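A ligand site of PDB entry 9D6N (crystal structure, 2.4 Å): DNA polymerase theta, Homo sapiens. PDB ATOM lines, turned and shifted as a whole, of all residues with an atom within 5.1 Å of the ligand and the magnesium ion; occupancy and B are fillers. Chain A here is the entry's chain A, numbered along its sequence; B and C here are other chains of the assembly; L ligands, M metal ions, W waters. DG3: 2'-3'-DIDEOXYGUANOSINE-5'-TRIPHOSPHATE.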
ATOM      1  N   ARG A 354      13.926  -2.761  33.073  1.00  0.00           N
ATOM      2  CA  ARG A 354      13.890  -2.407  31.663  1.00  0.00           C
ATOM      3  C   ARG A 354      12.470  -1.978  31.305  1.00  0.00           C
ATOM      4  O   ARG A 354      11.493  -2.412  31.927  1.00  0.00           O
ATOM      5  CB  ARG A 354      14.382  -3.543  30.757  1.00  0.00           C
ATOM      6  CG  ARG A 354      13.762  -4.930  30.919  1.00  0.00           C
ATOM      7  CD  ARG A 354      14.684  -5.972  30.257  1.00  0.00           C
ATOM      8  NE  ARG A 354      13.996  -6.810  29.285  1.00  0.00           N
ATOM      9  CZ  ARG A 354      14.601  -7.521  28.337  1.00  0.00           C
ATOM     10  NH1 ARG A 354      15.913  -7.494  28.192  1.00  0.00           N
ATOM     11  NH2 ARG A 354      13.868  -8.275  27.533  1.00  0.00           N
ATOM     12  N   ARG A 367      11.081  -9.431  13.544  1.00  0.00           N
ATOM     13  CA  ARG A 367      12.266  -9.228  12.735  1.00  0.00           C
ATOM     14  C   ARG A 367      11.951  -9.577  11.282  1.00  0.00           C
ATOM     15  O   ARG A 367      10.951 -10.228  10.972  1.00  0.00           O
ATOM     16  CB  ARG A 367      13.415 -10.093  13.252  1.00  0.00           C
ATOM     17  CG  ARG A 367      13.751  -9.895  14.724  1.00  0.00           C
ATOM     18  CD  ARG A 367      14.651 -11.001  15.264  1.00  0.00           C
ATOM     19  NE  ARG A 367      15.967 -11.024  14.636  1.00  0.00           N
ATOM     20  CZ  ARG A 367      17.007 -10.321  15.060  1.00  0.00           C
ATOM     21  NH1 ARG A 367      16.916  -9.500  16.102  1.00  0.00           N
ATOM     22  NH2 ARG A 367      18.170 -10.431  14.426  1.00  0.00           N
ATOM     23  N   ASP A 401      22.886   1.365  19.140  1.00  0.00           N
ATOM     24  CA  ASP A 401      22.745   0.048  19.747  1.00  0.00           C
ATOM     25  C   ASP A 401      23.981  -0.274  20.567  1.00  0.00           C
ATOM     26  O   ASP A 401      25.112  -0.164  20.073  1.00  0.00           O
ATOM     27  CB  ASP A 401      22.529  -1.012  18.656  1.00  0.00           C
ATOM     28  CG  ASP A 401      22.575  -2.436  19.191  1.00  0.00           C
ATOM     29  OD1 ASP A 401      21.644  -2.833  19.931  1.00  0.00           O
ATOM     30  OD2 ASP A 401      23.532  -3.162  18.848  1.00  0.00           O
ATOM     31  N   TYR A 402      23.771  -0.661  21.832  1.00  0.00           N
ATOM     32  CA  TYR A 402      24.850  -1.194  22.659  1.00  0.00           C
ATOM     33  C   TYR A 402      25.212  -2.589  22.146  1.00  0.00           C
ATOM     34  O   TYR A 402      24.405  -3.517  22.250  1.00  0.00           O
ATOM     35  CB  TYR A 402      24.437  -1.264  24.122  1.00  0.00           C
ATOM     36  CG  TYR A 402      24.581   0.027  24.903  1.00  0.00           C
ATOM     37  CD1 TYR A 402      25.824   0.634  25.051  1.00  0.00           C
ATOM     38  CD2 TYR A 402      23.483   0.609  25.527  1.00  0.00           C
ATOM     39  CE1 TYR A 402      25.952   1.807  25.779  1.00  0.00           C
ATOM     40  CE2 TYR A 402      23.602   1.784  26.250  1.00  0.00           C
ATOM     41  CZ  TYR A 402      24.843   2.385  26.375  1.00  0.00           C
ATOM     42  OH  TYR A 402      24.968   3.544  27.101  1.00  0.00           O
ATOM     43  N   GLN A 404      26.398  -6.025  22.373  1.00  0.00           N
ATOM     44  CA  GLN A 404      26.653  -7.062  23.376  1.00  0.00           C
ATOM     45  C   GLN A 404      26.733  -6.475  24.779  1.00  0.00           C
ATOM     46  O   GLN A 404      27.718  -6.627  25.501  1.00  0.00           O
ATOM     47  CB  GLN A 404      27.921  -7.846  23.034  1.00  0.00           C
ATOM     48  CG  GLN A 404      27.996  -8.308  21.581  1.00  0.00           C
ATOM     49  CD  GLN A 404      29.378  -8.143  20.986  1.00  0.00           C
ATOM     50  OE1 GLN A 404      30.098  -9.117  20.780  1.00  0.00           O
ATOM     51  NE2 GLN A 404      29.755  -6.900  20.711  1.00  0.00           N
ATOM     52  N   LEU A 405      25.654  -5.788  25.172  1.00  0.00           N
ATOM     53  CA  LEU A 405      25.640  -5.087  26.449  1.00  0.00           C
ATOM     54  C   LEU A 405      25.698  -6.056  27.624  1.00  0.00           C
ATOM     55  O   LEU A 405      26.570  -5.939  28.494  1.00  0.00           O
ATOM     56  CB  LEU A 405      24.409  -4.195  26.545  1.00  0.00           C
ATOM     57  CG  LEU A 405      24.289  -3.279  27.776  1.00  0.00           C
ATOM     58  CD1 LEU A 405      25.529  -2.403  27.929  1.00  0.00           C
ATOM     59  CD2 LEU A 405      23.040  -2.425  27.642  1.00  0.00           C
ATOM     60  N   GLU A 406      24.784  -7.029  27.667  1.00  0.00           N
ATOM     61  CA  GLU A 406      24.782  -7.946  28.804  1.00  0.00           C
ATOM     62  C   GLU A 406      26.031  -8.811  28.831  1.00  0.00           C
ATOM     63  O   GLU A 406      26.472  -9.241  29.905  1.00  0.00           O
ATOM     64  CB  GLU A 406      23.533  -8.832  28.765  1.00  0.00           C
ATOM     65  CG  GLU A 406      22.273  -8.120  29.247  1.00  0.00           C
ATOM     66  CD  GLU A 406      21.142  -9.086  29.497  1.00  0.00           C
ATOM     67  OE1 GLU A 406      21.410 -10.282  29.718  1.00  0.00           O
ATOM     68  OE2 GLU A 406      19.970  -8.653  29.463  1.00  0.00           O
ATOM     69  N   PHE A 430      27.158 -15.709  18.334  1.00  0.00           N
ATOM     70  CA  PHE A 430      25.968 -16.481  18.003  1.00  0.00           C
ATOM     71  C   PHE A 430      26.164 -17.267  16.703  1.00  0.00           C
ATOM     72  O   PHE A 430      25.724 -18.418  16.596  1.00  0.00           O
ATOM     73  CB  PHE A 430      24.759 -15.559  17.921  1.00  0.00           C
ATOM     74  CG  PHE A 430      24.563 -14.713  19.155  1.00  0.00           C
ATOM     75  CD1 PHE A 430      24.706 -15.261  20.423  1.00  0.00           C
ATOM     76  CD2 PHE A 430      24.259 -13.368  19.046  1.00  0.00           C
ATOM     77  CE1 PHE A 430      24.540 -14.492  21.551  1.00  0.00           C
ATOM     78  CE2 PHE A 430      24.096 -12.584  20.175  1.00  0.00           C
ATOM     79  CZ  PHE A 430      24.232 -13.145  21.425  1.00  0.00           C
ATOM     80  N   ARG A 450      20.686 -18.017  13.583  1.00  0.00           N
ATOM     81  CA  ARG A 450      21.407 -17.193  14.548  1.00  0.00           C
ATOM     82  C   ARG A 450      20.552 -16.898  15.770  1.00  0.00           C
ATOM     83  O   ARG A 450      21.044 -16.913  16.908  1.00  0.00           O
ATOM     84  CB  ARG A 450      21.873 -15.884  13.891  1.00  0.00           C
ATOM     85  CG  ARG A 450      22.781 -15.035  14.758  1.00  0.00           C
ATOM     86  CD  ARG A 450      23.178 -13.752  14.040  1.00  0.00           C
ATOM     87  NE  ARG A 450      24.056 -12.908  14.848  1.00  0.00           N
ATOM     88  CZ  ARG A 450      23.628 -11.951  15.663  1.00  0.00           C
ATOM     89  NH1 ARG A 450      22.331 -11.698  15.804  1.00  0.00           N
ATOM     90  NH2 ARG A 450      24.510 -11.235  16.342  1.00  0.00           N
ATOM     91  N   GLN A 451      19.251 -16.625  15.559  1.00  0.00           N
ATOM     92  CA  GLN A 451      18.349 -16.425  16.682  1.00  0.00           C
ATOM     93  C   GLN A 451      18.235 -17.677  17.537  1.00  0.00           C
ATOM     94  O   GLN A 451      18.124 -17.592  18.767  1.00  0.00           O
ATOM     95  CB  GLN A 451      16.976 -15.981  16.181  1.00  0.00           C
ATOM     96  CG  GLN A 451      16.923 -14.549  15.666  1.00  0.00           C
ATOM     97  CD  GLN A 451      17.178 -13.535  16.769  1.00  0.00           C
ATOM     98  OE1 GLN A 451      18.244 -12.934  16.833  1.00  0.00           O
ATOM     99  NE2 GLN A 451      16.191 -13.342  17.630  1.00  0.00           N
ATOM    100  N   LYS A 454      21.347 -17.698  19.523  1.00  0.00           N
ATOM    101  CA  LYS A 454      21.336 -16.632  20.522  1.00  0.00           C
ATOM    102  C   LYS A 454      20.623 -17.091  21.787  1.00  0.00           C
ATOM    103  O   LYS A 454      21.130 -16.906  22.902  1.00  0.00           O
ATOM    104  CB  LYS A 454      20.670 -15.383  19.944  1.00  0.00           C
ATOM    105  CG  LYS A 454      20.561 -14.245  20.948  1.00  0.00           C
ATOM    106  CD  LYS A 454      19.808 -13.062  20.352  1.00  0.00           C
ATOM    107  CE  LYS A 454      20.551 -12.467  19.168  1.00  0.00           C
ATOM    108  NZ  LYS A 454      19.835 -11.301  18.581  1.00  0.00           N
ATOM    109  N   GLN A 455      19.439 -17.697  21.634  1.00  0.00           N
ATOM    110  CA  GLN A 455      18.715 -18.194  22.804  1.00  0.00           C
ATOM    111  C   GLN A 455      19.447 -19.352  23.459  1.00  0.00           C
ATOM    112  O   GLN A 455      19.369 -19.514  24.681  1.00  0.00           O
ATOM    113  CB  GLN A 455      17.300 -18.607  22.397  1.00  0.00           C
ATOM    114  CG  GLN A 455      16.478 -17.466  21.804  1.00  0.00           C
ATOM    115  CD  GLN A 455      15.008 -17.544  22.170  1.00  0.00           C
ATOM    116  OE1 GLN A 455      14.255 -18.345  21.607  1.00  0.00           O
ATOM    117  NE2 GLN A 455      14.591 -16.717  23.114  1.00  0.00           N
ATOM    118  N   TYR A 458      22.391 -17.386  25.632  1.00  0.00           N
ATOM    119  CA  TYR A 458      21.939 -16.808  26.888  1.00  0.00           C
ATOM    120  C   TYR A 458      21.249 -17.840  27.769  1.00  0.00           C
ATOM    121  O   TYR A 458      21.302 -17.727  28.999  1.00  0.00           O
ATOM    122  CB  TYR A 458      21.006 -15.624  26.614  1.00  0.00           C
ATOM    123  CG  TYR A 458      21.685 -14.437  25.966  1.00  0.00           C
ATOM    124  CD1 TYR A 458      22.718 -13.762  26.613  1.00  0.00           C
ATOM    125  CD2 TYR A 458      21.299 -13.992  24.706  1.00  0.00           C
ATOM    126  CE1 TYR A 458      23.347 -12.668  26.026  1.00  0.00           C
ATOM    127  CE2 TYR A 458      21.925 -12.897  24.102  1.00  0.00           C
ATOM    128  CZ  TYR A 458      22.949 -12.250  24.778  1.00  0.00           C
ATOM    129  OH  TYR A 458      23.574 -11.169  24.190  1.00  0.00           O
ATOM    130  N   GLY A 459      20.626 -18.852  27.177  1.00  0.00           N
ATOM    131  CA  GLY A 459      20.026 -19.909  27.968  1.00  0.00           C
ATOM    132  C   GLY A 459      21.042 -20.653  28.820  1.00  0.00           C
ATOM    133  O   GLY A 459      20.873 -20.801  30.025  1.00  0.00           O
ATOM    134  N   TYR A 462      22.530 -18.427  31.559  1.00  0.00           N
ATOM    135  CA  TYR A 462      21.623 -18.130  32.649  1.00  0.00           C
ATOM    136  C   TYR A 462      20.959 -19.376  33.231  1.00  0.00           C
ATOM    137  O   TYR A 462      19.883 -19.270  33.843  1.00  0.00           O
ATOM    138  CB  TYR A 462      20.579 -17.110  32.207  1.00  0.00           C
ATOM    139  CG  TYR A 462      21.168 -15.747  31.901  1.00  0.00           C
ATOM    140  CD1 TYR A 462      21.869 -15.042  32.873  1.00  0.00           C
ATOM    141  CD2 TYR A 462      21.016 -15.161  30.650  1.00  0.00           C
ATOM    142  CE1 TYR A 462      22.412 -13.801  32.602  1.00  0.00           C
ATOM    143  CE2 TYR A 462      21.552 -13.925  30.368  1.00  0.00           C
ATOM    144  CZ  TYR A 462      22.249 -13.249  31.355  1.00  0.00           C
ATOM    145  OH  TYR A 462      22.784 -12.005  31.080  1.00  0.00           O
ATOM    146  N   ASN A 541      20.707 -13.498  36.583  1.00  0.00           N
ATOM    147  CA  ASN A 541      20.193 -12.787  35.427  1.00  0.00           C
ATOM    148  C   ASN A 541      19.809 -11.352  35.788  1.00  0.00           C
ATOM    149  O   ASN A 541      20.021 -10.430  34.983  1.00  0.00           O
ATOM    150  CB  ASN A 541      19.005 -13.537  34.833  1.00  0.00           C
ATOM    151  CG  ASN A 541      18.392 -12.810  33.656  1.00  0.00           C
ATOM    152  OD1 ASN A 541      17.394 -12.097  33.811  1.00  0.00           O
ATOM    153  ND2 ASN A 541      18.979 -12.971  32.478  1.00  0.00           N
ATOM    154  N   GLN A 545      21.017  -8.336  33.491  1.00  0.00           N
ATOM    155  CA  GLN A 545      19.956  -7.680  32.741  1.00  0.00           C
ATOM    156  C   GLN A 545      19.535  -6.370  33.412  1.00  0.00           C
ATOM    157  O   GLN A 545      19.283  -5.366  32.730  1.00  0.00           O
ATOM    158  CB  GLN A 545      18.757  -8.616  32.588  1.00  0.00           C
ATOM    159  CG  GLN A 545      17.624  -8.034  31.757  1.00  0.00           C
ATOM    160  CD  GLN A 545      16.390  -8.925  31.756  1.00  0.00           C
ATOM    161  OE1 GLN A 545      15.351  -8.564  32.304  1.00  0.00           O
ATOM    162  NE2 GLN A 545      16.509 -10.086  31.136  1.00  0.00           N
ATOM    163  N   LEU A 600      14.577  -0.302  22.994  1.00  0.00           N
ATOM    164  CA  LEU A 600      14.593  -1.725  22.656  1.00  0.00           C
ATOM    165  C   LEU A 600      15.580  -2.486  23.536  1.00  0.00           C
ATOM    166  O   LEU A 600      16.296  -3.369  23.067  1.00  0.00           O
ATOM    167  CB  LEU A 600      14.912  -1.930  21.178  1.00  0.00           C
ATOM    168  CG  LEU A 600      13.769  -1.654  20.201  1.00  0.00           C
ATOM    169  CD1 LEU A 600      14.299  -1.423  18.793  1.00  0.00           C
ATOM    170  CD2 LEU A 600      12.783  -2.813  20.226  1.00  0.00           C
ATOM    171  N   ASP A 602      18.424  -2.730  24.554  1.00  0.00           N
ATOM    172  CA  ASP A 602      19.815  -2.321  24.394  1.00  0.00           C
ATOM    173  C   ASP A 602      19.984  -1.397  23.190  1.00  0.00           C
ATOM    174  O   ASP A 602      21.092  -1.287  22.648  1.00  0.00           O
ATOM    175  CB  ASP A 602      20.751  -3.536  24.252  1.00  0.00           C
ATOM    176  CG  ASP A 602      20.521  -4.325  22.967  1.00  0.00           C
ATOM    177  OD1 ASP A 602      19.502  -4.094  22.287  1.00  0.00           O
ATOM    178  OD2 ASP A 602      21.380  -5.166  22.627  1.00  0.00           O
ATOM    179  P    DC B  10      15.071 -25.018  32.158  1.00  0.00           P
ATOM    180  OP1  DC B  10      13.930 -25.084  31.214  1.00  0.00           O
ATOM    181  OP2  DC B  10      16.035 -26.144  32.224  1.00  0.00           O
ATOM    182  O5'  DC B  10      15.916 -23.679  31.897  1.00  0.00           O
ATOM    183  C5'  DC B  10      15.312 -22.408  32.157  1.00  0.00           C
ATOM    184  C4'  DC B  10      16.377 -21.333  32.358  1.00  0.00           C
ATOM    185  O4'  DC B  10      17.184 -21.225  31.165  1.00  0.00           O
ATOM    186  C3'  DC B  10      15.834 -19.930  32.605  1.00  0.00           C
ATOM    187  O3'  DC B  10      15.592 -19.732  33.987  1.00  0.00           O
ATOM    188  C2'  DC B  10      16.976 -19.052  32.111  1.00  0.00           C
ATOM    189  C1'  DC B  10      17.532 -19.868  30.940  1.00  0.00           C
ATOM    190  N1   DC B  10      16.999 -19.451  29.594  1.00  0.00           N
ATOM    191  C2   DC B  10      17.291 -18.186  29.072  1.00  0.00           C
ATOM    192  O2   DC B  10      17.992 -17.406  29.737  1.00  0.00           O
ATOM    193  N3   DC B  10      16.802 -17.842  27.859  1.00  0.00           N
ATOM    194  C4   DC B  10      16.047 -18.704  27.169  1.00  0.00           C
ATOM    195  N4   DC B  10      15.594 -18.318  25.976  1.00  0.00           N
ATOM    196  C5   DC B  10      15.741 -20.001  27.679  1.00  0.00           C
ATOM    197  C6   DC B  10      16.230 -20.330  28.876  1.00  0.00           C
ATOM    198  P    DG B  11      14.187 -19.125  34.482  1.00  0.00           P
ATOM    199  OP1  DG B  11      14.071 -19.380  35.933  1.00  0.00           O
ATOM    200  OP2  DG B  11      13.139 -19.627  33.568  1.00  0.00           O
ATOM    201  O5'  DG B  11      14.329 -17.551  34.236  1.00  0.00           O
ATOM    202  C5'  DG B  11      15.316 -16.809  34.921  1.00  0.00           C
ATOM    203  C4'  DG B  11      15.520 -15.454  34.269  1.00  0.00           C
ATOM    204  O4'  DG B  11      16.011 -15.638  32.918  1.00  0.00           O
ATOM    205  C3'  DG B  11      14.253 -14.638  34.083  1.00  0.00           C
ATOM    206  O3'  DG B  11      13.951 -13.926  35.279  1.00  0.00           O
ATOM    207  C2'  DG B  11      14.655 -13.676  32.956  1.00  0.00           C
ATOM    208  C1'  DG B  11      15.652 -14.512  32.143  1.00  0.00           C
ATOM    209  N9   DG B  11      15.125 -14.955  30.858  1.00  0.00           N
ATOM    210  C8   DG B  11      14.646 -16.206  30.539  1.00  0.00           C
ATOM    211  N7   DG B  11      14.236 -16.308  29.306  1.00  0.00           N
ATOM    212  C5   DG B  11      14.457 -15.041  28.768  1.00  0.00           C
ATOM    213  C6   DG B  11      14.205 -14.546  27.463  1.00  0.00           C
ATOM    214  O6   DG B  11      13.726 -15.149  26.482  1.00  0.00           O
ATOM    215  N1   DG B  11      14.570 -13.210  27.340  1.00  0.00           N
ATOM    216  C2   DG B  11      15.109 -12.447  28.352  1.00  0.00           C
ATOM    217  N2   DG B  11      15.390 -11.173  28.057  1.00  0.00           N
ATOM    218  N3   DG B  11      15.341 -12.899  29.576  1.00  0.00           N
ATOM    219  C4   DG B  11      14.990 -14.202  29.711  1.00  0.00           C
ATOM    220  P    DC C  14      14.191  -8.705  18.582  1.00  0.00           P
ATOM    221  OP1  DC C  14      14.855  -7.880  17.548  1.00  0.00           O
ATOM    222  OP2  DC C  14      14.353 -10.172  18.543  1.00  0.00           O
ATOM    223  O5'  DC C  14      14.640  -8.205  20.044  1.00  0.00           O
ATOM    224  C5'  DC C  14      14.506  -6.828  20.395  1.00  0.00           C
ATOM    225  C4'  DC C  14      14.637  -6.634  21.894  1.00  0.00           C
ATOM    226  O4'  DC C  14      13.928  -7.699  22.599  1.00  0.00           O
ATOM    227  C3'  DC C  14      16.064  -6.635  22.444  1.00  0.00           C
ATOM    228  C2'  DC C  14      16.203  -8.018  23.070  1.00  0.00           C
ATOM    229  C1'  DC C  14      14.780  -8.278  23.554  1.00  0.00           C
ATOM    230  N1   DC C  14      14.452  -9.730  23.632  1.00  0.00           N
ATOM    231  C2   DC C  14      14.527 -10.392  24.863  1.00  0.00           C
ATOM    232  O2   DC C  14      14.848  -9.753  25.866  1.00  0.00           O
ATOM    233  N3   DC C  14      14.232 -11.727  24.909  1.00  0.00           N
ATOM    234  C4   DC C  14      13.885 -12.371  23.787  1.00  0.00           C
ATOM    235  N4   DC C  14      13.606 -13.682  23.884  1.00  0.00           N
ATOM    236  C5   DC C  14      13.813 -11.708  22.526  1.00  0.00           C
ATOM    237  C6   DC C  14      14.105 -10.402  22.496  1.00  0.00           C
HETATM  238  PG  DG3 L   1      22.497  -8.488  18.298  1.00  0.00           P
HETATM  239  O1G DG3 L   1      21.171  -7.756  18.417  1.00  0.00           O
HETATM  240  O2G DG3 L   1      23.716  -7.657  18.645  1.00  0.00           O
HETATM  241  O3G DG3 L   1      22.640  -9.328  17.033  1.00  0.00           O
HETATM  242  O3B DG3 L   1      22.461  -9.649  19.575  1.00  0.00           O
HETATM  243  PB  DG3 L   1      22.373  -9.363  21.158  1.00  0.00           P
HETATM  244  O1B DG3 L   1      23.588  -8.639  21.680  1.00  0.00           O
HETATM  245  O2B DG3 L   1      21.852 -10.546  21.907  1.00  0.00           O
HETATM  246  O3A DG3 L   1      21.150  -8.220  21.101  1.00  0.00           O
HETATM  247  PA  DG3 L   1      19.556  -8.516  21.249  1.00  0.00           P
HETATM  248  O1A DG3 L   1      18.793  -7.243  21.044  1.00  0.00           O
HETATM  249  O2A DG3 L   1      19.141  -9.753  20.524  1.00  0.00           O
HETATM  250  O5' DG3 L   1      19.609  -8.888  22.860  1.00  0.00           O
HETATM  251  C5' DG3 L   1      19.582  -7.862  23.823  1.00  0.00           C
HETATM  252  C4' DG3 L   1      19.587  -8.491  25.199  1.00  0.00           C
HETATM  253  O4' DG3 L   1      18.360  -9.167  25.472  1.00  0.00           O
HETATM  254  C3' DG3 L   1      20.637  -9.589  25.339  1.00  0.00           C
HETATM  255  C2' DG3 L   1      20.066 -10.376  26.512  1.00  0.00           C
HETATM  256  C1' DG3 L   1      18.563 -10.288  26.272  1.00  0.00           C
HETATM  257  N9  DG3 L   1      18.070 -11.493  25.587  1.00  0.00           N
HETATM  258  C8  DG3 L   1      17.708 -11.648  24.271  1.00  0.00           C
HETATM  259  N7  DG3 L   1      17.320 -12.855  23.996  1.00  0.00           N
HETATM  260  C5  DG3 L   1      17.423 -13.537  25.179  1.00  0.00           C
HETATM  261  C6  DG3 L   1      17.139 -14.906  25.503  1.00  0.00           C
HETATM  262  O6  DG3 L   1      16.714 -15.800  24.789  1.00  0.00           O
HETATM  263  N1  DG3 L   1      17.396 -15.157  26.855  1.00  0.00           N
HETATM  264  C2  DG3 L   1      17.867 -14.259  27.767  1.00  0.00           C
HETATM  265  N2  DG3 L   1      18.055 -14.701  29.017  1.00  0.00           N
HETATM  266  N3  DG3 L   1      18.124 -13.008  27.462  1.00  0.00           N
HETATM  267  C4  DG3 L   1      17.893 -12.707  26.180  1.00  0.00           C
HETATM  268 MG    MG M   1      22.033  -6.083  20.376  1.00  0.00          MG
HETATM  269  O   HOH W   1      16.249 -13.837  21.511  1.00  0.00           O
HETATM  270  O   HOH W   2      18.646 -11.568  30.016  1.00  0.00           O
HETATM  271  O   HOH W   3      16.755 -11.306  19.898  1.00  0.00           O
HETATM  272  O   HOH W   4      22.637  -5.260  17.050  1.00  0.00           O
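The side-chain amide nitrogen (NE2) of Gln 455 lies within hydrogen-bond range of an oxygen (O6) of the ligand, at 2.9 Å. The guanidinium group (NH1) of Arg 450 lies within salt-bridge range of an oxygen (O3G) of the ligand, at 2.7 Å. N2 of the ligand lies within hydrogen-bond range of O2 of DC 10 of chain B (2.8 Å). An oxygen (O2A) of the ligand is in salt-bridge range of the side-chain amino group (NZ) of Lys 454, 2.6 Å away. An oxygen (O2B) of the ligand lies within hydrogen-bond range of the side-chain hydroxyl of Tyr 458, at 2.9 Å. A nitrogen (N2) of the ligand sits close to N3 of DG 11 of chain B (3.3 Å).
N4 of DC 10 of chain B lies within hydrogen-bond range of NE2 of Gln 455 (3.4 Å). N3 of DG 11 of chain B lies within hydrogen-bond range of NE2 of Gln 545 (3.4 Å). N2 of DG 11 of chain B sits close to O2 of DC 14 of chain C (2.7 Å). N2 of DG 11 of chain B sits at hydrogen-bond distance from the guanidinium group (NH2) of Arg 354, at 3.3 Å. The side-chain amide oxygen of Gln 451 is in hydrogen-bond range of the side-chain amino group of Lys 454 (2.9 Å). N4 of DC 14 of chain C is in hydrogen-bond range of the side-chain amide nitrogen (NE2) of Gln 455, at 3.3 Å. The backbone carbonyl oxygen of Asp 602 sits at hydrogen-bond distance from the backbone NH of Tyr 402. The side-chain amide nitrogen of Gln 545 lies within hydrogen-bond range of the side-chain amide oxygen of Asn 541.
N3 of DC 14 of chain C lies close to a nitrogen (N7) of the ligand, 3.4 Å away. CA of Gln 404 touches O1B of the ligand, at 3.8 Å. Glu 406 touches the ligand. Phe 430 touches the ligand (CE2 to O3B, 3.4 Å). CD2 of Tyr 462 touches N2 of the ligand, 3.4 Å away. Asn 541 touches the ligand (ND2 to N2, 3.98 Å). Hydrophobic or aromatic side chains that line the ligand: Phe 430, Tyr 458 and Tyr 462.
Asp 401 touches the magnesium ion (OD1 to MG, 3.3 Å). O of Tyr 402 touches the magnesium ion (3.97 Å). Three residues have an atom within 4 Å of the magnesium ion: Asp 401, Tyr 402 and Asp 602.
The magnesium ion is bound by an oxygen (O3A) of the ligand (2.4 Å) and the side-chain carboxylate (OD2) of Asp 602 (2.5 Å). Slightly farther from the magnesium ion lies an oxygen (O1G) of the ligand (2.7 Å).
Water W3 lies within hydrogen-bond range of an oxygen (O2A) of the ligand (2.9 Å), OP2 of DC 14 of chain C (3.0 Å), the side-chain amide nitrogen (NE2) of Gln 451 (3.1 Å) and the side-chain amino group (NZ) of Lys 454 (3.3 Å). Water W2 lies within hydrogen-bond range of NE2 of Gln 545 (2.8 Å), ND2 of Asn 541 (2.9 Å), N3 of the ligand (3.0 Å) and OE1 of Glu 406 (3.1 Å). Water W4 lies within hydrogen-bond range of the side-chain carboxylate (OD2) of Asp 401 and an oxygen (O2G) of the ligand.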
